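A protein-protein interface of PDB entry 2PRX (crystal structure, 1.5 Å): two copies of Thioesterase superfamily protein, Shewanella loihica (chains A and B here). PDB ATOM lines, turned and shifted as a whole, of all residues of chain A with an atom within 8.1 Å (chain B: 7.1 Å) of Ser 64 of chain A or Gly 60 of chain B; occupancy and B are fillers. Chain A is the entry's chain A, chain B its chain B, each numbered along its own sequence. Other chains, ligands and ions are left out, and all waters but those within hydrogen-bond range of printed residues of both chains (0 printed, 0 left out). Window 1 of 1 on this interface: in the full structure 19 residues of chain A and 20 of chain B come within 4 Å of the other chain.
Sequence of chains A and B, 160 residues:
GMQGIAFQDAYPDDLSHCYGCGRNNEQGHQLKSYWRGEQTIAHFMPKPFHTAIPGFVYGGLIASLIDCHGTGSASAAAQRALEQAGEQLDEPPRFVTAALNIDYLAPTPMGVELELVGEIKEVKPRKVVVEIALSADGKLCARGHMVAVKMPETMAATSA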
ATOM      1  N   CYS A  18      -4.050 -20.643 -13.077  1.00  0.00           N
ATOM      2  CA  CYS A  18      -3.575 -19.547 -13.912  1.00  0.00           C
ATOM      3  C   CYS A  18      -3.764 -18.194 -13.222  1.00  0.00           C
ATOM      4  O   CYS A  18      -4.004 -18.190 -12.018  1.00  0.00           O
ATOM      5  CB  CYS A  18      -4.334 -19.631 -15.240  1.00  0.00           C
ATOM      6  SG  CYS A  18      -3.635 -18.624 -16.576  1.00  0.00           S
ATOM      7  N   TYR A  19      -3.623 -17.071 -13.897  1.00  0.00           N
ATOM      8  CA  TYR A  19      -3.849 -15.679 -13.593  1.00  0.00           C
ATOM      9  C   TYR A  19      -5.207 -15.235 -14.151  1.00  0.00           C
ATOM     10  O   TYR A  19      -5.547 -14.043 -14.163  1.00  0.00           O
ATOM     11  CB  TYR A  19      -2.700 -14.852 -14.154  1.00  0.00           C
ATOM     12  CG  TYR A  19      -2.689 -13.399 -13.767  1.00  0.00           C
ATOM     13  CD1 TYR A  19      -3.375 -12.939 -12.648  1.00  0.00           C
ATOM     14  CD2 TYR A  19      -2.004 -12.471 -14.538  1.00  0.00           C
ATOM     15  CE1 TYR A  19      -3.375 -11.613 -12.291  1.00  0.00           C
ATOM     16  CE2 TYR A  19      -1.995 -11.128 -14.190  1.00  0.00           C
ATOM     17  CZ  TYR A  19      -2.681 -10.708 -13.073  1.00  0.00           C
ATOM     18  OH  TYR A  19      -2.704  -9.392 -12.677  1.00  0.00           O
ATOM     19  N   GLY A  20      -5.964 -16.207 -14.621  1.00  0.00           N
ATOM     20  CA  GLY A  20      -7.354 -16.018 -15.012  1.00  0.00           C
ATOM     21  C   GLY A  20      -8.287 -16.303 -13.842  1.00  0.00           C
ATOM     22  O   GLY A  20      -8.771 -17.411 -13.606  1.00  0.00           O
ATOM     23  N   LEU A  31      -8.208 -12.745 -13.460  1.00  0.00           N
ATOM     24  CA  LEU A  31      -9.220 -12.124 -14.321  1.00  0.00           C
ATOM     25  C   LEU A  31     -10.568 -12.820 -14.203  1.00  0.00           C
ATOM     26  O   LEU A  31     -10.618 -14.047 -14.234  1.00  0.00           O
ATOM     27  CB  LEU A  31      -8.754 -12.113 -15.774  1.00  0.00           C
ATOM     28  CG  LEU A  31      -9.194 -10.947 -16.670  1.00  0.00           C
ATOM     29  CD1 LEU A  31      -9.023  -9.588 -16.053  1.00  0.00           C
ATOM     30  CD2 LEU A  31      -8.435 -11.024 -17.996  1.00  0.00           C
ATOM     31  N   HIS A  50       3.002  -2.568 -11.300  1.00  0.00           N
ATOM     32  CA  HIS A  50       2.908  -3.079 -12.666  1.00  0.00           C
ATOM     33  C   HIS A  50       3.219  -2.032 -13.721  1.00  0.00           C
ATOM     34  O   HIS A  50       2.545  -1.940 -14.750  1.00  0.00           O
ATOM     35  CB  HIS A  50       1.497  -3.629 -12.941  1.00  0.00           C
ATOM     36  CG  HIS A  50       1.320  -5.052 -12.531  1.00  0.00           C
ATOM     37  ND1 HIS A  50       0.794  -5.389 -11.294  1.00  0.00           N
ATOM     38  CD2 HIS A  50       1.566  -6.222 -13.145  1.00  0.00           C
ATOM     39  CE1 HIS A  50       0.731  -6.701 -11.174  1.00  0.00           C
ATOM     40  NE2 HIS A  50       1.200  -7.235 -12.292  1.00  0.00           N
ATOM     41  N   TYR A  58       2.545  -1.694 -17.569  1.00  0.00           N
ATOM     42  CA  TYR A  58       3.394  -2.665 -18.240  1.00  0.00           C
ATOM     43  C   TYR A  58       2.692  -3.367 -19.385  1.00  0.00           C
ATOM     44  O   TYR A  58       1.606  -3.921 -19.268  1.00  0.00           O
ATOM     45  CB  TYR A  58       3.868  -3.665 -17.174  1.00  0.00           C
ATOM     46  CG  TYR A  58       4.789  -4.714 -17.742  1.00  0.00           C
ATOM     47  CD1 TYR A  58       5.755  -4.356 -18.670  1.00  0.00           C
ATOM     48  CD2 TYR A  58       4.662  -6.030 -17.348  1.00  0.00           C
ATOM     49  CE1 TYR A  58       6.599  -5.313 -19.200  1.00  0.00           C
ATOM     50  CE2 TYR A  58       5.503  -6.986 -17.869  1.00  0.00           C
ATOM     51  CZ  TYR A  58       6.460  -6.619 -18.789  1.00  0.00           C
ATOM     52  OH  TYR A  58       7.293  -7.588 -19.296  1.00  0.00           O
ATOM     53  N   GLY A  59       3.322  -3.387 -20.552  1.00  0.00           N
ATOM     54  CA  GLY A  59       2.870  -4.114 -21.709  1.00  0.00           C
ATOM     55  C   GLY A  59       2.700  -5.604 -21.525  1.00  0.00           C
ATOM     56  O   GLY A  59       1.726  -6.145 -22.079  1.00  0.00           O
ATOM     57  N   GLY A  60       3.562  -6.298 -20.783  1.00  0.00           N
ATOM     58  CA  GLY A  60       3.435  -7.716 -20.496  1.00  0.00           C
ATOM     59  C   GLY A  60       2.101  -8.064 -19.791  1.00  0.00           C
ATOM     60  O   GLY A  60       1.511  -9.058 -20.137  1.00  0.00           O
ATOM     61  N   LEU A  61       1.800  -7.233 -18.800  1.00  0.00           N
ATOM     62  CA  LEU A  61       0.536  -7.346 -18.080  1.00  0.00           C
ATOM     63  C   LEU A  61      -0.623  -7.192 -19.049  1.00  0.00           C
ATOM     64  O   LEU A  61      -1.549  -8.000 -19.062  1.00  0.00           O
ATOM     65  CB  LEU A  61       0.437  -6.297 -16.954  1.00  0.00           C
ATOM     66  CG  LEU A  61      -0.896  -6.380 -16.195  1.00  0.00           C
ATOM     67  CD1 LEU A  61      -1.105  -7.749 -15.562  1.00  0.00           C
ATOM     68  CD2 LEU A  61      -0.951  -5.297 -15.137  1.00  0.00           C
ATOM     69  N   ILE A  62      -0.587  -6.166 -19.881  1.00  0.00           N
ATOM     70  CA  ILE A  62      -1.628  -5.953 -20.905  1.00  0.00           C
ATOM     71  C   ILE A  62      -1.709  -7.153 -21.813  1.00  0.00           C
ATOM     72  O   ILE A  62      -2.765  -7.755 -22.022  1.00  0.00           O
ATOM     73  CB  ILE A  62      -1.324  -4.626 -21.636  1.00  0.00           C
ATOM     74  CG1 ILE A  62      -1.375  -3.457 -20.668  1.00  0.00           C
ATOM     75  CG2 ILE A  62      -2.223  -4.411 -22.835  1.00  0.00           C
ATOM     76  CD1 ILE A  62      -1.431  -2.066 -21.247  1.00  0.00           C
ATOM     77  N   ALA A  63      -0.603  -7.623 -22.377  1.00  0.00           N
ATOM     78  CA  ALA A  63      -0.657  -8.820 -23.201  1.00  0.00           C
ATOM     79  C   ALA A  63      -1.161 -10.031 -22.420  1.00  0.00           C
ATOM     80  O   ALA A  63      -1.792 -10.899 -23.048  1.00  0.00           O
ATOM     81  CB  ALA A  63       0.710  -9.148 -23.793  1.00  0.00           C
ATOM     82  N   SER A  64      -0.886 -10.066 -21.128  1.00  0.00           N
ATOM     83  CA  SER A  64      -1.293 -11.173 -20.273  1.00  0.00           C
ATOM     84  C   SER A  64      -2.823 -11.201 -20.148  1.00  0.00           C
ATOM     85  O   SER A  64      -3.367 -12.309 -20.251  1.00  0.00           O
ATOM     86  CB  SER A  64      -0.708 -11.138 -18.867  1.00  0.00           C
ATOM     87  OG  SER A  64       0.703 -11.087 -18.834  1.00  0.00           O
ATOM     88  N   LEU A  65      -3.419 -10.034 -19.934  1.00  0.00           N
ATOM     89  CA  LEU A  65      -4.890  -9.945 -19.731  1.00  0.00           C
ATOM     90  C   LEU A  65      -5.622 -10.204 -21.020  1.00  0.00           C
ATOM     91  O   LEU A  65      -6.759 -10.738 -21.072  1.00  0.00           O
ATOM     92  CB  LEU A  65      -5.240  -8.586 -19.133  1.00  0.00           C
ATOM     93  CG  LEU A  65      -4.590  -8.250 -17.777  1.00  0.00           C
ATOM     94  CD1 LEU A  65      -4.741  -6.779 -17.453  1.00  0.00           C
ATOM     95  CD2 LEU A  65      -5.196  -9.113 -16.679  1.00  0.00           C
ATOM     96  N   ILE A  66      -5.073  -9.875 -22.178  1.00  0.00           N
ATOM     97  CA  ILE A  66      -5.775 -10.215 -23.419  1.00  0.00           C
ATOM     98  C   ILE A  66      -5.838 -11.726 -23.629  1.00  0.00           C
ATOM     99  O   ILE A  66      -6.855 -12.300 -24.036  1.00  0.00           O
ATOM    100  CB  ILE A  66      -5.100  -9.535 -24.619  1.00  0.00           C
ATOM    101  CG1 ILE A  66      -5.458  -8.051 -24.751  1.00  0.00           C
ATOM    102  CG2 ILE A  66      -5.385 -10.307 -25.883  1.00  0.00           C
ATOM    103  CD1 ILE A  66      -4.391  -7.274 -25.496  1.00  0.00           C
ATOM    104  N   ASP A  67      -4.721 -12.379 -23.331  1.00  0.00           N
ATOM    105  CA  ASP A  67      -4.593 -13.826 -23.432  1.00  0.00           C
ATOM    106  C   ASP A  67      -5.619 -14.552 -22.579  1.00  0.00           C
ATOM    107  O   ASP A  67      -6.294 -15.475 -23.023  1.00  0.00           O
ATOM    108  CB  ASP A  67      -3.188 -14.221 -22.992  1.00  0.00           C
ATOM    109  CG  ASP A  67      -2.843 -15.687 -23.062  1.00  0.00           C
ATOM    110  OD1 ASP A  67      -3.696 -16.507 -23.439  1.00  0.00           O
ATOM    111  OD2 ASP A  67      -1.670 -16.003 -22.739  1.00  0.00           O
ATOM    112  N   CYS A  68      -5.724 -14.150 -21.306  1.00  0.00           N
ATOM    113  CA  CYS A  68      -6.636 -14.955 -20.473  1.00  0.00           C
ATOM    114  C   CYS A  68      -8.061 -14.523 -20.771  1.00  0.00           C
ATOM    115  O   CYS A  68      -8.995 -15.324 -20.671  1.00  0.00           O
ATOM    116  CB  CYS A  68      -6.253 -14.850 -18.999  1.00  0.00           C
ATOM    117  SG  CYS A  68      -4.643 -15.574 -18.568  1.00  0.00           S
ATOM    118  N   HIS A  69      -8.282 -13.262 -21.144  1.00  0.00           N
ATOM    119  CA  HIS A  69      -9.680 -12.918 -21.469  1.00  0.00           C
ATOM    120  C   HIS A  69     -10.096 -13.618 -22.752  1.00  0.00           C
ATOM    121  O   HIS A  69     -11.239 -14.053 -22.900  1.00  0.00           O
ATOM    122  CB  HIS A  69      -9.832 -11.406 -21.575  1.00  0.00           C
ATOM    123  CG  HIS A  69     -11.205 -10.959 -22.000  1.00  0.00           C
ATOM    124  ND1 HIS A  69     -12.326 -11.163 -21.213  1.00  0.00           N
ATOM    125  CD2 HIS A  69     -11.628 -10.327 -23.107  1.00  0.00           C
ATOM    126  CE1 HIS A  69     -13.375 -10.661 -21.849  1.00  0.00           C
ATOM    127  NE2 HIS A  69     -12.993 -10.143 -23.001  1.00  0.00           N
ATOM    128  N   GLY A  70      -9.162 -13.731 -23.693  1.00  0.00           N
ATOM    129  CA  GLY A  70      -9.394 -14.278 -25.019  1.00  0.00           C
ATOM    130  C   GLY A  70      -9.654 -15.770 -24.990  1.00  0.00           C
ATOM    131  O   GLY A  70     -10.439 -16.350 -25.746  1.00  0.00           O
ATOM    132  N   THR A  71      -8.943 -16.420 -24.067  1.00  0.00           N
ATOM    133  CA  THR A  71      -9.100 -17.848 -23.849  1.00  0.00           C
ATOM    134  C   THR A  71     -10.405 -18.060 -23.085  1.00  0.00           C
ATOM    135  O   THR A  71     -11.160 -18.961 -23.421  1.00  0.00           O
ATOM    136  CB  THR A  71      -7.923 -18.462 -23.083  1.00  0.00           C
ATOM    137  OG1 THR A  71      -6.765 -18.501 -23.927  1.00  0.00           O
ATOM    138  CG2 THR A  71      -8.236 -19.902 -22.702  1.00  0.00           C
ATOM    139  N   THR A  97      -3.988 -20.742 -26.120  1.00  0.00           N
ATOM    140  CA  THR A  97      -3.681 -19.790 -27.181  1.00  0.00           C
ATOM    141  C   THR A  97      -2.763 -20.454 -28.197  1.00  0.00           C
ATOM    142  O   THR A  97      -1.778 -21.063 -27.789  1.00  0.00           O
ATOM    143  CB  THR A  97      -3.001 -18.520 -26.638  1.00  0.00           C
ATOM    144  OG1 THR A  97      -3.887 -17.792 -25.780  1.00  0.00           O
ATOM    145  CG2 THR A  97      -2.624 -17.601 -27.791  1.00  0.00           C
ATOM    146  N   LEU A 100      -1.385 -15.258 -30.767  1.00  0.00           N
ATOM    147  CA  LEU A 100      -1.880 -14.013 -30.210  1.00  0.00           C
ATOM    148  C   LEU A 100      -1.009 -12.890 -30.803  1.00  0.00           C
ATOM    149  O   LEU A 100       0.195 -12.892 -30.527  1.00  0.00           O
ATOM    150  CB  LEU A 100      -1.853 -13.918 -28.700  1.00  0.00           C
ATOM    151  CG  LEU A 100      -2.494 -12.703 -28.025  1.00  0.00           C
ATOM    152  CD1 LEU A 100      -3.954 -12.506 -28.425  1.00  0.00           C
ATOM    153  CD2 LEU A 100      -2.401 -12.849 -26.509  1.00  0.00           C
ATOM    154  N   ILE A 102      -0.794  -8.733 -31.235  1.00  0.00           N
ATOM    155  CA  ILE A 102      -1.201  -7.561 -30.493  1.00  0.00           C
ATOM    156  C   ILE A 102      -0.483  -6.302 -30.994  1.00  0.00           C
ATOM    157  O   ILE A 102       0.745  -6.303 -31.039  1.00  0.00           O
ATOM    158  CB  ILE A 102      -0.946  -7.720 -28.986  1.00  0.00           C
ATOM    159  CG1 ILE A 102      -1.519  -9.006 -28.389  1.00  0.00           C
ATOM    160  CG2 ILE A 102      -1.454  -6.512 -28.216  1.00  0.00           C
ATOM    161  CD1 ILE A 102      -1.132  -9.279 -26.955  1.00  0.00           C
ATOM    162  N   TYR A 104      -0.174  -2.306 -30.157  1.00  0.00           N
ATOM    163  CA  TYR A 104      -0.182  -1.353 -29.064  1.00  0.00           C
ATOM    164  C   TYR A 104      -0.494   0.037 -29.584  1.00  0.00           C
ATOM    165  O   TYR A 104       0.321   0.763 -30.127  1.00  0.00           O
ATOM    166  CB  TYR A 104       1.170  -1.451 -28.356  1.00  0.00           C
ATOM    167  CG  TYR A 104       1.299  -2.756 -27.603  1.00  0.00           C
ATOM    168  CD1 TYR A 104       0.831  -2.869 -26.296  1.00  0.00           C
ATOM    169  CD2 TYR A 104       1.853  -3.869 -28.191  1.00  0.00           C
ATOM    170  CE1 TYR A 104       0.943  -4.067 -25.613  1.00  0.00           C
ATOM    171  CE2 TYR A 104       1.976  -5.067 -27.522  1.00  0.00           C
ATOM    172  CZ  TYR A 104       1.513  -5.165 -26.221  1.00  0.00           C
ATOM    173  OH  TYR A 104       1.637  -6.361 -25.553  1.00  0.00           O
ATOM    174  N   LEU A 116     -11.634  -4.835 -20.800  1.00  0.00           N
ATOM    175  CA  LEU A 116     -11.389  -5.789 -21.851  1.00  0.00           C
ATOM    176  C   LEU A 116     -12.689  -6.358 -22.424  1.00  0.00           C
ATOM    177  O   LEU A 116     -13.435  -6.969 -21.659  1.00  0.00           O
ATOM    178  CB  LEU A 116     -10.567  -6.975 -21.325  1.00  0.00           C
ATOM    179  CG  LEU A 116      -9.071  -6.691 -21.143  1.00  0.00           C
ATOM    180  CD1 LEU A 116      -8.841  -6.147 -19.745  1.00  0.00           C
ATOM    181  CD2 LEU A 116      -8.247  -7.936 -21.413  1.00  0.00           C
ATOM    182  N   LEU A 134      -8.375  -3.778 -25.337  1.00  0.00           N
ATOM    183  CA  LEU A 134      -8.201  -3.235 -23.997  1.00  0.00           C
ATOM    184  C   LEU A 134      -8.197  -1.707 -24.039  1.00  0.00           C
ATOM    185  O   LEU A 134      -7.465  -1.166 -24.869  1.00  0.00           O
ATOM    186  CB  LEU A 134      -6.914  -3.722 -23.344  1.00  0.00           C
ATOM    187  CG  LEU A 134      -6.650  -3.253 -21.912  1.00  0.00           C
ATOM    188  CD1 LEU A 134      -6.034  -4.378 -21.098  1.00  0.00           C
ATOM    189  CD2 LEU A 134      -5.746  -2.029 -21.861  1.00  0.00           C
ATOM    190  N   MET A 146      -6.559 -13.260 -31.589  1.00  0.00           N
ATOM    191  CA  MET A 146      -6.314 -14.540 -31.007  1.00  0.00           C
ATOM    192  C   MET A 146      -6.957 -15.674 -31.803  1.00  0.00           C
ATOM    193  O   MET A 146      -8.084 -15.530 -32.269  1.00  0.00           O
ATOM    194  CB  MET A 146      -6.882 -14.594 -29.569  1.00  0.00           C
ATOM    195  CG  MET A 146      -6.980 -16.030 -29.092  1.00  0.00           C
ATOM    196  SD  MET A 146      -7.402 -16.152 -27.218  1.00  0.00           S
ATOM    197  CE  MET A 146      -5.562 -15.770 -26.755  1.00  0.00           C
ATOM    198  N   VAL B  57       4.218 -23.496 -17.798  1.00  0.00           N
ATOM    199  CA  VAL B  57       4.439 -22.083 -17.580  1.00  0.00           C
ATOM    200  C   VAL B  57       3.332 -21.205 -18.187  1.00  0.00           C
ATOM    201  O   VAL B  57       2.920 -21.457 -19.323  1.00  0.00           O
ATOM    202  CB  VAL B  57       5.778 -21.562 -18.141  1.00  0.00           C
ATOM    203  CG1 VAL B  57       5.872 -20.054 -17.996  1.00  0.00           C
ATOM    204  CG2 VAL B  57       6.904 -22.255 -17.400  1.00  0.00           C
ATOM    205  N   TYR B  58       2.925 -20.237 -17.370  1.00  0.00           N
ATOM    206  CA  TYR B  58       1.898 -19.277 -17.741  1.00  0.00           C
ATOM    207  C   TYR B  58       2.255 -18.596 -19.056  1.00  0.00           C
ATOM    208  O   TYR B  58       3.278 -17.934 -19.176  1.00  0.00           O
ATOM    209  CB  TYR B  58       1.731 -18.243 -16.619  1.00  0.00           C
ATOM    210  CG  TYR B  58       0.796 -17.125 -17.001  1.00  0.00           C
ATOM    211  CD1 TYR B  58      -0.487 -17.454 -17.421  1.00  0.00           C
ATOM    212  CD2 TYR B  58       1.157 -15.788 -16.954  1.00  0.00           C
ATOM    213  CE1 TYR B  58      -1.387 -16.474 -17.784  1.00  0.00           C
ATOM    214  CE2 TYR B  58       0.265 -14.801 -17.315  1.00  0.00           C
ATOM    215  CZ  TYR B  58      -1.006 -15.153 -17.728  1.00  0.00           C
ATOM    216  OH  TYR B  58      -1.890 -14.162 -18.091  1.00  0.00           O
ATOM    217  N   GLY B  59       1.385 -18.763 -20.051  1.00  0.00           N
ATOM    218  CA  GLY B  59       1.609 -18.217 -21.364  1.00  0.00           C
ATOM    219  C   GLY B  59       1.752 -16.718 -21.478  1.00  0.00           C
ATOM    220  O   GLY B  59       2.294 -16.256 -22.496  1.00  0.00           O
ATOM    221  N   GLY B  60       1.301 -15.931 -20.520  1.00  0.00           N
ATOM    222  CA  GLY B  60       1.413 -14.497 -20.480  1.00  0.00           C
ATOM    223  C   GLY B  60       2.800 -14.079 -19.986  1.00  0.00           C
ATOM    224  O   GLY B  60       3.309 -13.054 -20.436  1.00  0.00           O
ATOM    225  N   LEU B  61       3.375 -14.850 -19.064  1.00  0.00           N
ATOM    226  CA  LEU B  61       4.785 -14.578 -18.707  1.00  0.00           C
ATOM    227  C   LEU B  61       5.634 -14.608 -19.979  1.00  0.00           C
ATOM    228  O   LEU B  61       6.313 -13.623 -20.286  1.00  0.00           O
ATOM    229  CB  LEU B  61       5.352 -15.541 -17.677  1.00  0.00           C
ATOM    230  CG  LEU B  61       6.867 -15.396 -17.405  1.00  0.00           C
ATOM    231  CD1 LEU B  61       7.162 -14.054 -16.766  1.00  0.00           C
ATOM    232  CD2 LEU B  61       7.369 -16.530 -16.534  1.00  0.00           C
ATOM    233  N   ILE B  62       5.580 -15.721 -20.692  1.00  0.00           N
ATOM    234  CA  ILE B  62       6.280 -15.941 -21.966  1.00  0.00           C
ATOM    235  C   ILE B  62       6.155 -14.728 -22.854  1.00  0.00           C
ATOM    236  O   ILE B  62       7.113 -14.228 -23.443  1.00  0.00           O
ATOM    237  CB  ILE B  62       5.739 -17.214 -22.658  1.00  0.00           C
ATOM    238  CG1 ILE B  62       5.866 -18.463 -21.794  1.00  0.00           C
ATOM    239  CG2 ILE B  62       6.398 -17.410 -24.014  1.00  0.00           C
ATOM    240  CD1 ILE B  62       5.552 -19.749 -22.526  1.00  0.00           C
ATOM    241  N   ALA B  63       4.967 -14.154 -22.976  1.00  0.00           N
ATOM    242  CA  ALA B  63       4.831 -12.919 -23.724  1.00  0.00           C
ATOM    243  C   ALA B  63       5.526 -11.740 -23.041  1.00  0.00           C
ATOM    244  O   ALA B  63       6.084 -10.908 -23.771  1.00  0.00           O
ATOM    245  CB  ALA B  63       3.358 -12.624 -23.922  1.00  0.00           C
ATOM    246  N   SER B  64       5.448 -11.695 -21.713  1.00  0.00           N
ATOM    247  CA  SER B  64       6.146 -10.684 -20.929  1.00  0.00           C
ATOM    248  C   SER B  64       7.653 -10.730 -21.207  1.00  0.00           C
ATOM    249  O   SER B  64       8.180  -9.642 -21.481  1.00  0.00           O
ATOM    250  CB  SER B  64       5.891 -10.838 -19.424  1.00  0.00           C
ATOM    251  OG  SER B  64       4.585 -10.364 -19.104  1.00  0.00           O
ATOM    252  N   LEU B  65       8.245 -11.911 -21.155  1.00  0.00           N
ATOM    253  CA  LEU B  65       9.671 -12.116 -21.438  1.00  0.00           C
ATOM    254  C   LEU B  65       9.978 -11.859 -22.899  1.00  0.00           C
ATOM    255  O   LEU B  65      11.022 -11.270 -23.259  1.00  0.00           O
ATOM    256  CB  LEU B  65      10.117 -13.519 -21.001  1.00  0.00           C
ATOM    257  CG  LEU B  65       9.984 -13.829 -19.508  1.00  0.00           C
ATOM    258  CD1 LEU B  65      10.244 -15.286 -19.175  1.00  0.00           C
ATOM    259  CD2 LEU B  65      10.889 -12.937 -18.674  1.00  0.00           C
ATOM    260  N   ILE B  66       9.145 -12.274 -23.847  1.00  0.00           N
ATOM    261  CA  ILE B  66       9.500 -12.060 -25.259  1.00  0.00           C
ATOM    262  C   ILE B  66       9.528 -10.583 -25.586  1.00  0.00           C
ATOM    263  O   ILE B  66      10.311 -10.022 -26.351  1.00  0.00           O
ATOM    264  CB  ILE B  66       8.494 -12.824 -26.149  1.00  0.00           C
ATOM    265  CG1 ILE B  66       8.767 -14.332 -26.252  1.00  0.00           C
ATOM    266  CG2 ILE B  66       8.391 -12.177 -27.517  1.00  0.00           C
ATOM    267  CD1 ILE B  66       7.532 -15.122 -26.682  1.00  0.00           C
ATOM    268  N   ILE B 102       2.718 -13.570 -31.320  1.00  0.00           N
ATOM    269  CA  ILE B 102       3.337 -14.769 -30.759  1.00  0.00           C
ATOM    270  C   ILE B 102       2.596 -16.045 -31.185  1.00  0.00           C
ATOM    271  O   ILE B 102       1.382 -16.117 -30.989  1.00  0.00           O
ATOM    272  CB  ILE B 102       3.447 -14.707 -29.230  1.00  0.00           C
ATOM    273  CG1 ILE B 102       3.983 -13.367 -28.721  1.00  0.00           C
ATOM    274  CG2 ILE B 102       4.300 -15.862 -28.717  1.00  0.00           C
ATOM    275  CD1 ILE B 102       4.110 -13.174 -27.229  1.00  0.00           C
ATOM    276  N   TYR B 104       2.538 -19.830 -30.138  1.00  0.00           N
ATOM    277  CA  TYR B 104       2.904 -20.762 -29.072  1.00  0.00           C
ATOM    278  C   TYR B 104       3.024 -22.160 -29.662  1.00  0.00           C
ATOM    279  O   TYR B 104       2.094 -22.880 -30.000  1.00  0.00           O
ATOM    280  CB  TYR B 104       1.916 -20.607 -27.919  1.00  0.00           C
ATOM    281  CG  TYR B 104       1.844 -19.155 -27.461  1.00  0.00           C
ATOM    282  CD1 TYR B 104       2.781 -18.597 -26.589  1.00  0.00           C
ATOM    283  CD2 TYR B 104       0.855 -18.312 -27.921  1.00  0.00           C
ATOM    284  CE1 TYR B 104       2.707 -17.280 -26.198  1.00  0.00           C
ATOM    285  CE2 TYR B 104       0.763 -16.990 -27.534  1.00  0.00           C
ATOM    286  CZ  TYR B 104       1.698 -16.462 -26.661  1.00  0.00           C
ATOM    287  OH  TYR B 104       1.606 -15.137 -26.277  1.00  0.00           O
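Ser 64 of chain A touches three residues of chain B.
Of chain A, only Ser 64 (3.6 Å) and Asp 67 (3.7 Å) come within 4 Å of Gly 60 of chain B.
Of chain A, only Asp 67 (3.7 Å) comes within 4 Å of Gly 59 of chain B.
Of the printed residues of chain A, Tyr 58 of chain B touches Cys 18, Tyr 19, Ser 64 and Cys 68.
Of the printed residues of chain B, Thr 97 of chain A touches Tyr 104 (3.5 Å).
Printed residues of chain B within 4 Å of Asp 67 of chain A: Gly 59 (3.7 Å) and Gly 60 (3.7 Å).
Leu 61 of chain B touches none of the printed residues of chain A.
The nearest printed residue of chain B that does not touch Leu 100 of chain A is Tyr 104 of chain B (4.2 Å).
The backbone carbonyl oxygen of Gly 60 of chain B lies within hydrogen-bond range of the side-chain hydroxyl of Ser 64 of chain B (3.3 Å).
The backbone NH (N) of Leu 31 of chain A lies within hydrogen-bond range of the backbone carbonyl oxygen (O) of Tyr 19 of chain A (3.0 Å).
OG1 of Thr 71 of chain A lies within hydrogen-bond range of OG1 of Thr 97 of chain A (3.5 Å).
OG1 of Thr 71 of chain A is in hydrogen-bond range of O of Asp 67 of chain A.
The backbone NH (N) of Tyr 58 of chain A lies within hydrogen-bond range of the backbone carbonyl oxygen (O) of His 50 of chain A (2.8 Å).
The backbone carbonyl oxygen of Gly 60 of chain A is in hydrogen-bond range of the side-chain hydroxyl of Ser 64 of chain A (2.5 Å).
Of the 26 printed residues of chain A, 9 touch a printed residue of chain B.
Printed residues of chain A that touch a printed residue of chain B: Cys 18, Tyr 19, Tyr 58, Gly 60, Ser 64, Asp 67, Cys 68, Thr 97 and Leu 100.
Printed residues of chain B that touch a printed residue of chain A: Tyr 58, Gly 59, Gly 60, Ser 64, Ile 102 and Tyr 104.
Hydrophobic or aromatic side chains of chain B within 4 Å of the printed part of chain A: Tyr 58, Ile 102 and Tyr 104.
Tyr 58 of chain A touches Ser 64 of chain B, and with the chains exchanged Ser 64 of chain A touches Tyr 58 of chain B.
Gly 60 of chain A touches Ser 64 of chain B, and with the chains exchanged Ser 64 of chain A touches Gly 60 of chain B.
Ser 64 of chain B touches its own counterpart, Ser 64 of chain A.
Cys 18 of chain A touches Tyr 58 of chain B (SG to CE1, 3.3 Å).
OH of Tyr 58 of chain B touches CD2 of Tyr 19 of chain A (3.9 Å).
OG of Ser 64 of chain A touches O of Gly 60 of chain B (3.6 Å).
OG of Ser 64 of chain B touches OG of Ser 64 of chain A, 3.96 Å away.
Asp 67 of chain A touches Gly 59 of chain B.
OD2 of Asp 67 of chain A touches N of Gly 60 of chain B, at 3.7 Å.
CE2 of Tyr 104 of chain B touches CG2 of Thr 97 of chain A, 3.5 Å away.
The backbone carbonyl oxygen (O) of Ser 64 of chain A lies within hydrogen-bond range of the side-chain hydroxyl (OH) of Tyr 58 of chain B (3.2 Å).
The backbone carbonyl oxygen (O) of Gly 60 of chain A sits close to the side-chain hydroxyl (OG) of Ser 64 of chain B (3.5 Å).
The backbone carbonyl oxygen (O) of Ser 64 of chain B is in hydrogen-bond range of the side-chain hydroxyl (OH) of Tyr 58 of chain A (3.1 Å).
N of Ile 102 of chain B lies within hydrogen-bond range of O of Leu 100 of chain A, at 2.7 Å.
The side-chain hydroxyl (OH) of Tyr 58 of chain B sits at hydrogen-bond distance from the side-chain sulfur (SG) of Cys 68 of chain A (3.1 Å).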
